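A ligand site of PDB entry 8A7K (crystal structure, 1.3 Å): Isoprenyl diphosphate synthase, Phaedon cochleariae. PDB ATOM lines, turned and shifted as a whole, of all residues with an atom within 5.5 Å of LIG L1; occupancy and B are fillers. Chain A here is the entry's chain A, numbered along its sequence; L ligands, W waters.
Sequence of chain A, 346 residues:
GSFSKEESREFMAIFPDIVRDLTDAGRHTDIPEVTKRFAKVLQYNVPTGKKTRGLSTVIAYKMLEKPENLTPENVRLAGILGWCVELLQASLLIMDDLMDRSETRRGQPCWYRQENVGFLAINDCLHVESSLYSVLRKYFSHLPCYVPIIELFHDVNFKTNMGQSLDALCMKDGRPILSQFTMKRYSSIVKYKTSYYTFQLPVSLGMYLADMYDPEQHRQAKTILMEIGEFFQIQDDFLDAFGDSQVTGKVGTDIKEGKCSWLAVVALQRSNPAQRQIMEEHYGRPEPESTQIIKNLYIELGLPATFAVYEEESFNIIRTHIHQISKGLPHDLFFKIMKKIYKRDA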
ATOM      1  N   GLY A  49      16.474  10.145   5.409  1.00  0.00           N
ATOM      2  CA  GLY A  49      17.438  10.179   4.324  1.00  0.00           C
ATOM      3  C   GLY A  49      18.647  11.043   4.656  1.00  0.00           C
ATOM      4  O   GLY A  49      18.800  11.448   5.823  1.00  0.00           O
ATOM      5  N   LYS A  50      19.480  11.300   3.662  1.00  0.00           N
ATOM      6  CA  LYS A  50      20.713  12.104   3.871  1.00  0.00           C
ATOM      7  C   LYS A  50      20.383  13.592   4.027  1.00  0.00           C
ATOM      8  O   LYS A  50      21.253  14.311   4.537  1.00  0.00           O
ATOM      9  CB  LYS A  50      21.668  11.849   2.729  1.00  0.00           C
ATOM     10  CG  LYS A  50      22.117  10.413   2.605  1.00  0.00           C
ATOM     11  CD  LYS A  50      23.023  10.202   1.439  1.00  0.00           C
ATOM     12  CE  LYS A  50      22.361  10.395   0.099  1.00  0.00           C
ATOM     13  NZ  LYS A  50      21.447   9.319  -0.167  1.00  0.00           N
ATOM     14  N   LYS A  51      19.225  14.036   3.548  1.00  0.00           N
ATOM     15  CA  LYS A  51      18.757  15.445   3.624  1.00  0.00           C
ATOM     16  C   LYS A  51      19.622  16.400   2.780  1.00  0.00           C
ATOM     17  O   LYS A  51      19.661  17.565   3.102  1.00  0.00           O
ATOM     18  CB  LYS A  51      18.540  15.851   5.093  1.00  0.00           C
ATOM     19  CG  LYS A  51      17.421  15.074   5.755  1.00  0.00           C
ATOM     20  CD  LYS A  51      17.316  15.233   7.241  1.00  0.00           C
ATOM     21  CE  LYS A  51      18.408  14.584   8.016  1.00  0.00           C
ATOM     22  NZ  LYS A  51      18.325  13.137   8.052  1.00  0.00           N
ATOM     23  N   ARG A  53      19.257  17.549  -0.256  1.00  0.00           N
ATOM     24  CA  ARG A  53      18.446  18.612  -0.925  1.00  0.00           C
ATOM     25  C   ARG A  53      18.051  19.718   0.065  1.00  0.00           C
ATOM     26  O   ARG A  53      18.174  20.911  -0.245  1.00  0.00           O
ATOM     27  CB  ARG A  53      17.219  17.995  -1.553  1.00  0.00           C
ATOM     28  CG  ARG A  53      17.445  16.993  -2.692  1.00  0.00           C
ATOM     29  CD  ARG A  53      16.232  16.173  -2.959  1.00  0.00           C
ATOM     30  NE  ARG A  53      16.489  15.093  -3.924  1.00  0.00           N
ATOM     31  CZ  ARG A  53      17.195  13.999  -3.685  1.00  0.00           C
ATOM     32  NH1 ARG A  53      17.648  13.746  -2.448  1.00  0.00           N
ATOM     33  NH2 ARG A  53      17.408  13.107  -4.638  1.00  0.00           N
ATOM     34  N   GLU A  86      12.311  18.292   0.956  1.00  0.00           N
ATOM     35  CA  GLU A  86      12.311  16.937   1.560  1.00  0.00           C
ATOM     36  C   GLU A  86      10.915  16.293   1.522  1.00  0.00           C
ATOM     37  O   GLU A  86      10.820  15.074   1.390  1.00  0.00           O
ATOM     38  CB  GLU A  86      12.923  16.955   2.955  1.00  0.00           C
ATOM     39  CG  GLU A  86      14.413  17.292   2.905  1.00  0.00           C
ATOM     40  CD  GLU A  86      15.323  16.282   2.217  1.00  0.00           C
ATOM     41  OE1 GLU A  86      14.956  15.074   2.137  1.00  0.00           O
ATOM     42  OE2 GLU A  86      16.434  16.713   1.760  1.00  0.00           O
ATOM     43  N   GLN A  89      10.586  15.084  -2.032  1.00  0.00           N
ATOM     44  CA  GLN A  89      11.393  13.843  -2.109  1.00  0.00           C
ATOM     45  C   GLN A  89      10.641  12.689  -1.467  1.00  0.00           C
ATOM     46  O   GLN A  89      10.523  11.592  -2.051  1.00  0.00           O
ATOM     47  CB  GLN A  89      12.738  14.057  -1.423  1.00  0.00           C
ATOM     48  CG  GLN A  89      13.597  12.809  -1.142  1.00  0.00           C
ATOM     49  CD  GLN A  89      14.191  12.204  -2.389  1.00  0.00           C
ATOM     50  OE1 GLN A  89      13.644  12.308  -3.498  1.00  0.00           O
ATOM     51  NE2 GLN A  89      15.370  11.531  -2.218  1.00  0.00           N
ATOM     52  N   LEU A  93       9.500   9.201  -3.393  1.00  0.00           N
ATOM     53  CA  LEU A  93      10.058   7.879  -3.051  1.00  0.00           C
ATOM     54  C   LEU A  93       8.933   6.890  -2.723  1.00  0.00           C
ATOM     55  O   LEU A  93       9.056   5.733  -3.059  1.00  0.00           O
ATOM     56  CB  LEU A  93      11.134   7.953  -1.987  1.00  0.00           C
ATOM     57  CG  LEU A  93      12.341   8.847  -2.343  1.00  0.00           C
ATOM     58  CD1 LEU A  93      13.383   8.724  -1.235  1.00  0.00           C
ATOM     59  CD2 LEU A  93      12.921   8.532  -3.723  1.00  0.00           C
ATOM     60  N   ARG A 105      13.801   0.800   1.650  1.00  0.00           N
ATOM     61  CA  ARG A 105      14.088   2.220   1.419  1.00  0.00           C
ATOM     62  C   ARG A 105      14.648   2.788   2.707  1.00  0.00           C
ATOM     63  O   ARG A 105      14.027   2.600   3.740  1.00  0.00           O
ATOM     64  CB  ARG A 105      12.810   2.947   1.051  1.00  0.00           C
ATOM     65  CG  ARG A 105      12.973   4.455   0.987  1.00  0.00           C
ATOM     66  CD  ARG A 105      13.856   5.017  -0.116  1.00  0.00           C
ATOM     67  NE  ARG A 105      13.299   4.769  -1.424  1.00  0.00           N
ATOM     68  CZ  ARG A 105      13.915   5.081  -2.555  1.00  0.00           C
ATOM     69  NH1 ARG A 105      15.123   5.618  -2.566  1.00  0.00           N
ATOM     70  NH2 ARG A 105      13.333   4.801  -3.720  1.00  0.00           N
ATOM     71  N   ARG A 106      15.783   3.458   2.633  1.00  0.00           N
ATOM     72  CA  ARG A 106      16.369   4.100   3.834  1.00  0.00           C
ATOM     73  C   ARG A 106      16.511   3.090   5.009  1.00  0.00           C
ATOM     74  O   ARG A 106      16.348   3.444   6.154  1.00  0.00           O
ATOM     75  CB  ARG A 106      15.603   5.356   4.241  1.00  0.00           C
ATOM     76  CG  ARG A 106      15.748   6.458   3.211  1.00  0.00           C
ATOM     77  CD  ARG A 106      14.749   7.578   3.474  1.00  0.00           C
ATOM     78  NE  ARG A 106      14.880   8.675   2.552  1.00  0.00           N
ATOM     79  CZ  ARG A 106      14.067   9.729   2.536  1.00  0.00           C
ATOM     80  NH1 ARG A 106      13.000   9.769   3.311  1.00  0.00           N
ATOM     81  NH2 ARG A 106      14.264  10.696   1.672  1.00  0.00           N
ATOM     82  N   LYS A 193      13.574  13.285 -14.467  1.00  0.00           N
ATOM     83  CA  LYS A 193      13.178  12.502 -13.258  1.00  0.00           C
ATOM     84  C   LYS A 193      13.969  12.852 -12.019  1.00  0.00           C
ATOM     85  O   LYS A 193      13.524  12.504 -10.925  1.00  0.00           O
ATOM     86  CB  LYS A 193      13.194  10.992 -13.494  1.00  0.00           C
ATOM     87  CG  LYS A 193      14.554  10.331 -13.467  1.00  0.00           C
ATOM     88  CD  LYS A 193      14.492   8.871 -13.241  1.00  0.00           C
ATOM     89  CE  LYS A 193      15.865   8.237 -13.236  1.00  0.00           C
ATOM     90  NZ  LYS A 193      15.812   6.776 -12.990  1.00  0.00           N
ATOM     91  N   THR A 194      15.153  13.496 -12.205  1.00  0.00           N
ATOM     92  CA  THR A 194      16.017  13.732 -11.051  1.00  0.00           C
ATOM     93  C   THR A 194      16.576  15.178 -11.014  1.00  0.00           C
ATOM     94  O   THR A 194      16.542  15.766  -9.937  1.00  0.00           O
ATOM     95  CB  THR A 194      17.152  12.715 -11.084  1.00  0.00           C
ATOM     96  OG1 THR A 194      16.600  11.462 -10.701  1.00  0.00           O
ATOM     97  CG2 THR A 194      18.307  13.098 -10.146  1.00  0.00           C
ATOM     98  N   TYR A 197      14.381  18.437  -9.643  1.00  0.00           N
ATOM     99  CA  TYR A 197      13.957  18.524  -8.229  1.00  0.00           C
ATOM    100  C   TYR A 197      15.114  18.337  -7.287  1.00  0.00           C
ATOM    101  O   TYR A 197      15.036  18.844  -6.135  1.00  0.00           O
ATOM    102  CB  TYR A 197      12.829  17.526  -7.901  1.00  0.00           C
ATOM    103  CG  TYR A 197      13.271  16.144  -7.443  1.00  0.00           C
ATOM    104  CD1 TYR A 197      13.536  15.106  -8.280  1.00  0.00           C
ATOM    105  CD2 TYR A 197      13.338  15.892  -6.087  1.00  0.00           C
ATOM    106  CE1 TYR A 197      13.870  13.835  -7.804  1.00  0.00           C
ATOM    107  CE2 TYR A 197      13.666  14.644  -5.582  1.00  0.00           C
ATOM    108  CZ  TYR A 197      13.982  13.613  -6.445  1.00  0.00           C
ATOM    109  OH  TYR A 197      14.279  12.352  -6.001  1.00  0.00           O
ATOM    110  N   THR A 198      16.163  17.646  -7.701  1.00  0.00           N
ATOM    111  CA  THR A 198      17.240  17.346  -6.746  1.00  0.00           C
ATOM    112  C   THR A 198      18.260  18.483  -6.709  1.00  0.00           C
ATOM    113  O   THR A 198      18.814  18.738  -5.627  1.00  0.00           O
ATOM    114  CB  THR A 198      17.914  16.001  -7.102  1.00  0.00           C
ATOM    115  OG1 THR A 198      16.929  14.951  -7.000  1.00  0.00           O
ATOM    116  CG2 THR A 198      19.086  15.695  -6.212  1.00  0.00           C
ATOM    117  N   PHE A 232      24.936  12.606 -10.719  1.00  0.00           N
ATOM    118  CA  PHE A 232      24.370  12.056  -9.465  1.00  0.00           C
ATOM    119  C   PHE A 232      23.496  10.823  -9.793  1.00  0.00           C
ATOM    120  O   PHE A 232      23.514   9.817  -9.047  1.00  0.00           O
ATOM    121  CB  PHE A 232      23.532  13.140  -8.763  1.00  0.00           C
ATOM    122  CG  PHE A 232      22.832  12.697  -7.526  1.00  0.00           C
ATOM    123  CD1 PHE A 232      23.526  12.617  -6.330  1.00  0.00           C
ATOM    124  CD2 PHE A 232      21.485  12.414  -7.530  1.00  0.00           C
ATOM    125  CE1 PHE A 232      22.887  12.229  -5.162  1.00  0.00           C
ATOM    126  CE2 PHE A 232      20.851  12.076  -6.369  1.00  0.00           C
ATOM    127  CZ  PHE A 232      21.546  11.975  -5.181  1.00  0.00           C
ATOM    128  N   GLN A 233      22.677  10.887 -10.864  1.00  0.00           N
ATOM    129  CA  GLN A 233      21.863   9.730 -11.253  1.00  0.00           C
ATOM    130  C   GLN A 233      22.707   8.554 -11.772  1.00  0.00           C
ATOM    131  O   GLN A 233      22.342   7.404 -11.498  1.00  0.00           O
ATOM    132  CB  GLN A 233      20.764  10.118 -12.220  1.00  0.00           C
ATOM    133  CG  GLN A 233      19.745   8.977 -12.478  1.00  0.00           C
ATOM    134  CD  GLN A 233      18.945   8.623 -11.238  1.00  0.00           C
ATOM    135  OE1 GLN A 233      18.447   9.503 -10.552  1.00  0.00           O
ATOM    136  NE2 GLN A 233      18.848   7.329 -10.988  1.00  0.00           N
ATOM    137  N   ASP A 236      23.674   6.892  -8.756  1.00  0.00           N
ATOM    138  CA  ASP A 236      22.549   6.084  -8.236  1.00  0.00           C
ATOM    139  C   ASP A 236      22.439   4.734  -8.964  1.00  0.00           C
ATOM    140  O   ASP A 236      22.135   3.707  -8.381  1.00  0.00           O
ATOM    141  CB  ASP A 236      21.249   6.862  -8.346  1.00  0.00           C
ATOM    142  CG  ASP A 236      20.122   6.118  -7.698  1.00  0.00           C
ATOM    143  OD1 ASP A 236      20.136   5.951  -6.457  1.00  0.00           O
ATOM    144  OD2 ASP A 236      19.175   5.705  -8.433  1.00  0.00           O
ATOM    145  N   LYS A 250      18.822   0.372   0.401  1.00  0.00           N
ATOM    146  CA  LYS A 250      17.833  -0.025  -0.608  1.00  0.00           C
ATOM    147  C   LYS A 250      18.407  -1.176  -1.430  1.00  0.00           C
ATOM    148  O   LYS A 250      19.592  -1.228  -1.753  1.00  0.00           O
ATOM    149  CB  LYS A 250      17.372   1.148  -1.477  1.00  0.00           C
ATOM    150  CG  LYS A 250      18.483   1.810  -2.302  1.00  0.00           C
ATOM    151  CD  LYS A 250      18.015   3.135  -2.887  1.00  0.00           C
ATOM    152  CE  LYS A 250      18.991   3.685  -3.899  1.00  0.00           C
ATOM    153  NZ  LYS A 250      18.582   5.006  -4.382  1.00  0.00           N
ATOM    154  N   ARG A 344      30.574   8.953  -3.349  1.00  0.00           N
ATOM    155  CA  ARG A 344      29.606   8.443  -2.366  1.00  0.00           C
ATOM    156  C   ARG A 344      29.306   6.946  -2.560  1.00  0.00           C
ATOM    157  O   ARG A 344      29.334   6.431  -3.672  1.00  0.00           O
ATOM    158  CB  ARG A 344      28.283   9.219  -2.403  1.00  0.00           C
ATOM    159  CG  ARG A 344      27.464   9.020  -3.660  1.00  0.00           C
ATOM    160  CD  ARG A 344      26.357  10.069  -3.743  1.00  0.00           C
ATOM    161  NE  ARG A 344      25.463   9.913  -4.901  1.00  0.00           N
ATOM    162  CZ  ARG A 344      24.360   9.223  -4.900  1.00  0.00           C
ATOM    163  NH1 ARG A 344      23.910   8.638  -3.820  1.00  0.00           N
ATOM    164  NH2 ARG A 344      23.639   9.094  -6.016  1.00  0.00           N
ATOM    165  N   ALA A 346      26.445   5.783  -0.811  1.00  0.00           N
ATOM    166  CA  ALA A 346      25.031   5.774  -0.411  1.00  0.00           C
ATOM    167  C   ALA A 346      24.380   7.066  -0.888  1.00  0.00           C
ATOM    168  O   ALA A 346      23.141   7.116  -0.922  1.00  0.00           O
ATOM    169  CB  ALA A 346      24.933   5.713   1.080  1.00  0.00           C
ATOM    170  OXT ALA A 346      25.099   8.070  -1.194  1.00  0.00           O
HETATM  171  C1  LIG L   1      17.324   9.082  -4.118  1.00  0.00           C
HETATM  172  O1  LIG L   1      17.941  10.252  -3.591  1.00  0.00           O
HETATM  173  C2  LIG L   1      16.665   9.367  -5.450  1.00  0.00           C
HETATM  174  C3  LIG L   1      17.547   9.920  -6.539  1.00  0.00           C
HETATM  175  C4  LIG L   1      17.244  11.034  -7.189  1.00  0.00           C
HETATM  176  C5  LIG L   1      18.841   9.209  -6.790  1.00  0.00           C
HETATM  177  P1  LIG L   1      18.957  10.169  -2.395  1.00  0.00           P
HETATM  178  O2  LIG L   1      20.008   9.160  -2.669  1.00  0.00           O
HETATM  179  O3  LIG L   1      19.429  11.558  -2.181  1.00  0.00           O
HETATM  180  O4  LIG L   1      18.063   9.612  -1.184  1.00  0.00           O
HETATM  181  P2  LIG L   1      17.743  10.108   0.337  1.00  0.00           P
HETATM  182  O5  LIG L   1      17.277   8.836   1.003  1.00  0.00           O
HETATM  183  O6  LIG L   1      19.013  10.587   0.874  1.00  0.00           O
HETATM  184  O7  LIG L   1      16.659  11.130   0.280  1.00  0.00           O
HETATM  185  O1  LG2 L   2      14.917   6.553 -10.472  1.00  0.00           O
HETATM  186  P1  LG2 L   2      15.135   5.479  -9.403  1.00  0.00           P
HETATM  187  O2  LG2 L   2      13.763   4.625  -9.295  1.00  0.00           O
HETATM  188  O3  LG2 L   2      16.433   4.643  -9.648  1.00  0.00           O
HETATM  189  C1  LG2 L   2      15.476   6.277  -7.796  1.00  0.00           C
HETATM  190  P2  LG2 L   2      15.781   5.051  -6.452  1.00  0.00           P
HETATM  191  O4  LG2 L   2      17.051   4.354  -6.842  1.00  0.00           O
HETATM  192  O5  LG2 L   2      14.645   4.072  -6.357  1.00  0.00           O
HETATM  193  O6  LG2 L   2      15.957   5.773  -5.157  1.00  0.00           O
HETATM  194  O7  LG2 L   2      16.635   7.105  -7.914  1.00  0.00           O
HETATM  195  C2  LG2 L   2      14.303   7.176  -7.413  1.00  0.00           C
HETATM  196  N1  LG2 L   2      14.050   8.324  -8.279  1.00  0.00           N
HETATM  197  C3  LG2 L   2      14.895   9.240  -8.725  1.00  0.00           C
HETATM  198  N2  LG2 L   2      14.301  10.118  -9.542  1.00  0.00           N
HETATM  199  C4  LG2 L   2      12.972   9.737  -9.535  1.00  0.00           C
HETATM  200  C5  LG2 L   2      12.773   8.665  -8.791  1.00  0.00           C
HETATM  201  O   HOH W   1      21.556  13.150  -1.890  1.00  0.00           O
HETATM  202  O   HOH W   2      21.371   7.786  -4.775  1.00  0.00           O
HETATM  203  O   HOH W   3      16.740  13.039   2.305  1.00  0.00           O
HETATM  204  O   HOH W   4      17.055   6.519  -0.480  1.00  0.00           O
HETATM  205  O   HOH W   5      19.615  13.243   0.388  1.00  0.00           O
HETATM  206  O   HOH W   6      19.356   7.570   2.171  1.00  0.00           O
HETATM  207  O   HOH W   7      19.282   6.600  -2.121  1.00  0.00           O
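NH1 of Arg 53 is in salt-bridge range of O3 of LIG L1 (2.8 Å).
O6 of LIG L1 sits at hydrogen-bond distance from N of Lys 50.
NE2 of Gln 89 lies within hydrogen-bond range of O7 of LIG L1.
The side-chain amino group (NZ) of Lys 250 lies within salt-bridge range of an oxygen (O6) of LG2 L2, at 2.8 Å.
O7 of LIG L1 lies within salt-bridge range of NH2 of Arg 106, at 2.8 Å.
An oxygen (O1) of LG2 L2 lies within salt-bridge range of the side-chain amino group (NZ) of Lys 193.
OG1 of Thr 194 sits at hydrogen-bond distance from N2 of LG2 L2 (2.9 Å).
NH1 of Arg 105 lies within salt-bridge range of O6 of LG2 L2 (2.7 Å).
O2 of LIG L1 lies within salt-bridge range of NZ of Lys 50, 2.9 Å away.
OG1 of Thr 194 lies within hydrogen-bond range of OE1 of Gln 233.
O of Phe 232 lies within hydrogen-bond range of NH2 of Arg 344 (3.1 Å).
The chain-end carboxylate of Ala 346 lies within salt-bridge range of the side-chain amino group of Lys 50, at 2.9 Å.
OD2 of Asp 236 lies close to NE2 of Gln 233, 3.0 Å away.
The backbone carbonyl oxygen (O) of Gly 49 sits at hydrogen-bond distance from the side-chain amino group (NZ) of Lys 51 (2.8 Å).
OG1 of Thr 198 is in hydrogen-bond range of O of Thr 194.
The side-chain hydroxyl (OH) of Tyr 197 sits at hydrogen-bond distance from the side-chain amide oxygen (OE1) of Gln 89 (2.6 Å).
The side-chain amide nitrogen (NE2) of Gln 89 lies close to the guanidinium group (NH1) of Arg 53 (3.2 Å).
Merely in contact with LIG L1: Tyr 197 (3.5 Å), Asp 236 (3.5 Å), Phe 232 (3.5 Å), Gly 49 (3.6 Å), Thr 194 (3.6 Å), Gln 233 (3.8 Å) and Thr 198 (3.9 Å).
Hydrophobic or aromatic side chains within 4 Å of LIG L1: Phe 232.
Of the 19 residues printed, 11 come within 4 Å of LIG L1.
Water W7 bridges an oxygen (O2) of LIG L1 and the side-chain amino group of Lys 250.
Water W4 bridges O5 of LIG L1 (2.8 Å) and NH1 of Arg 105 (3.0 Å).
Water W5 lies within hydrogen-bond range of O6 of LIG L1 (2.8 Å), N of Lys 51 (3.3 Å) and NH1 of Arg 53 (3.5 Å).
Water W3 lies within hydrogen-bond range of OE1 of Glu 86 (2.7 Å), O7 of LIG L1 (2.8 Å), N of Lys 51 (3.0 Å) and NH2 of Arg 106 (3.5 Å).
Water W2 lies within hydrogen-bond range of OD1 of Asp 236 (2.8 Å), NH1 of Arg 344 (2.8 Å) and O2 of LIG L1 (2.9 Å).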
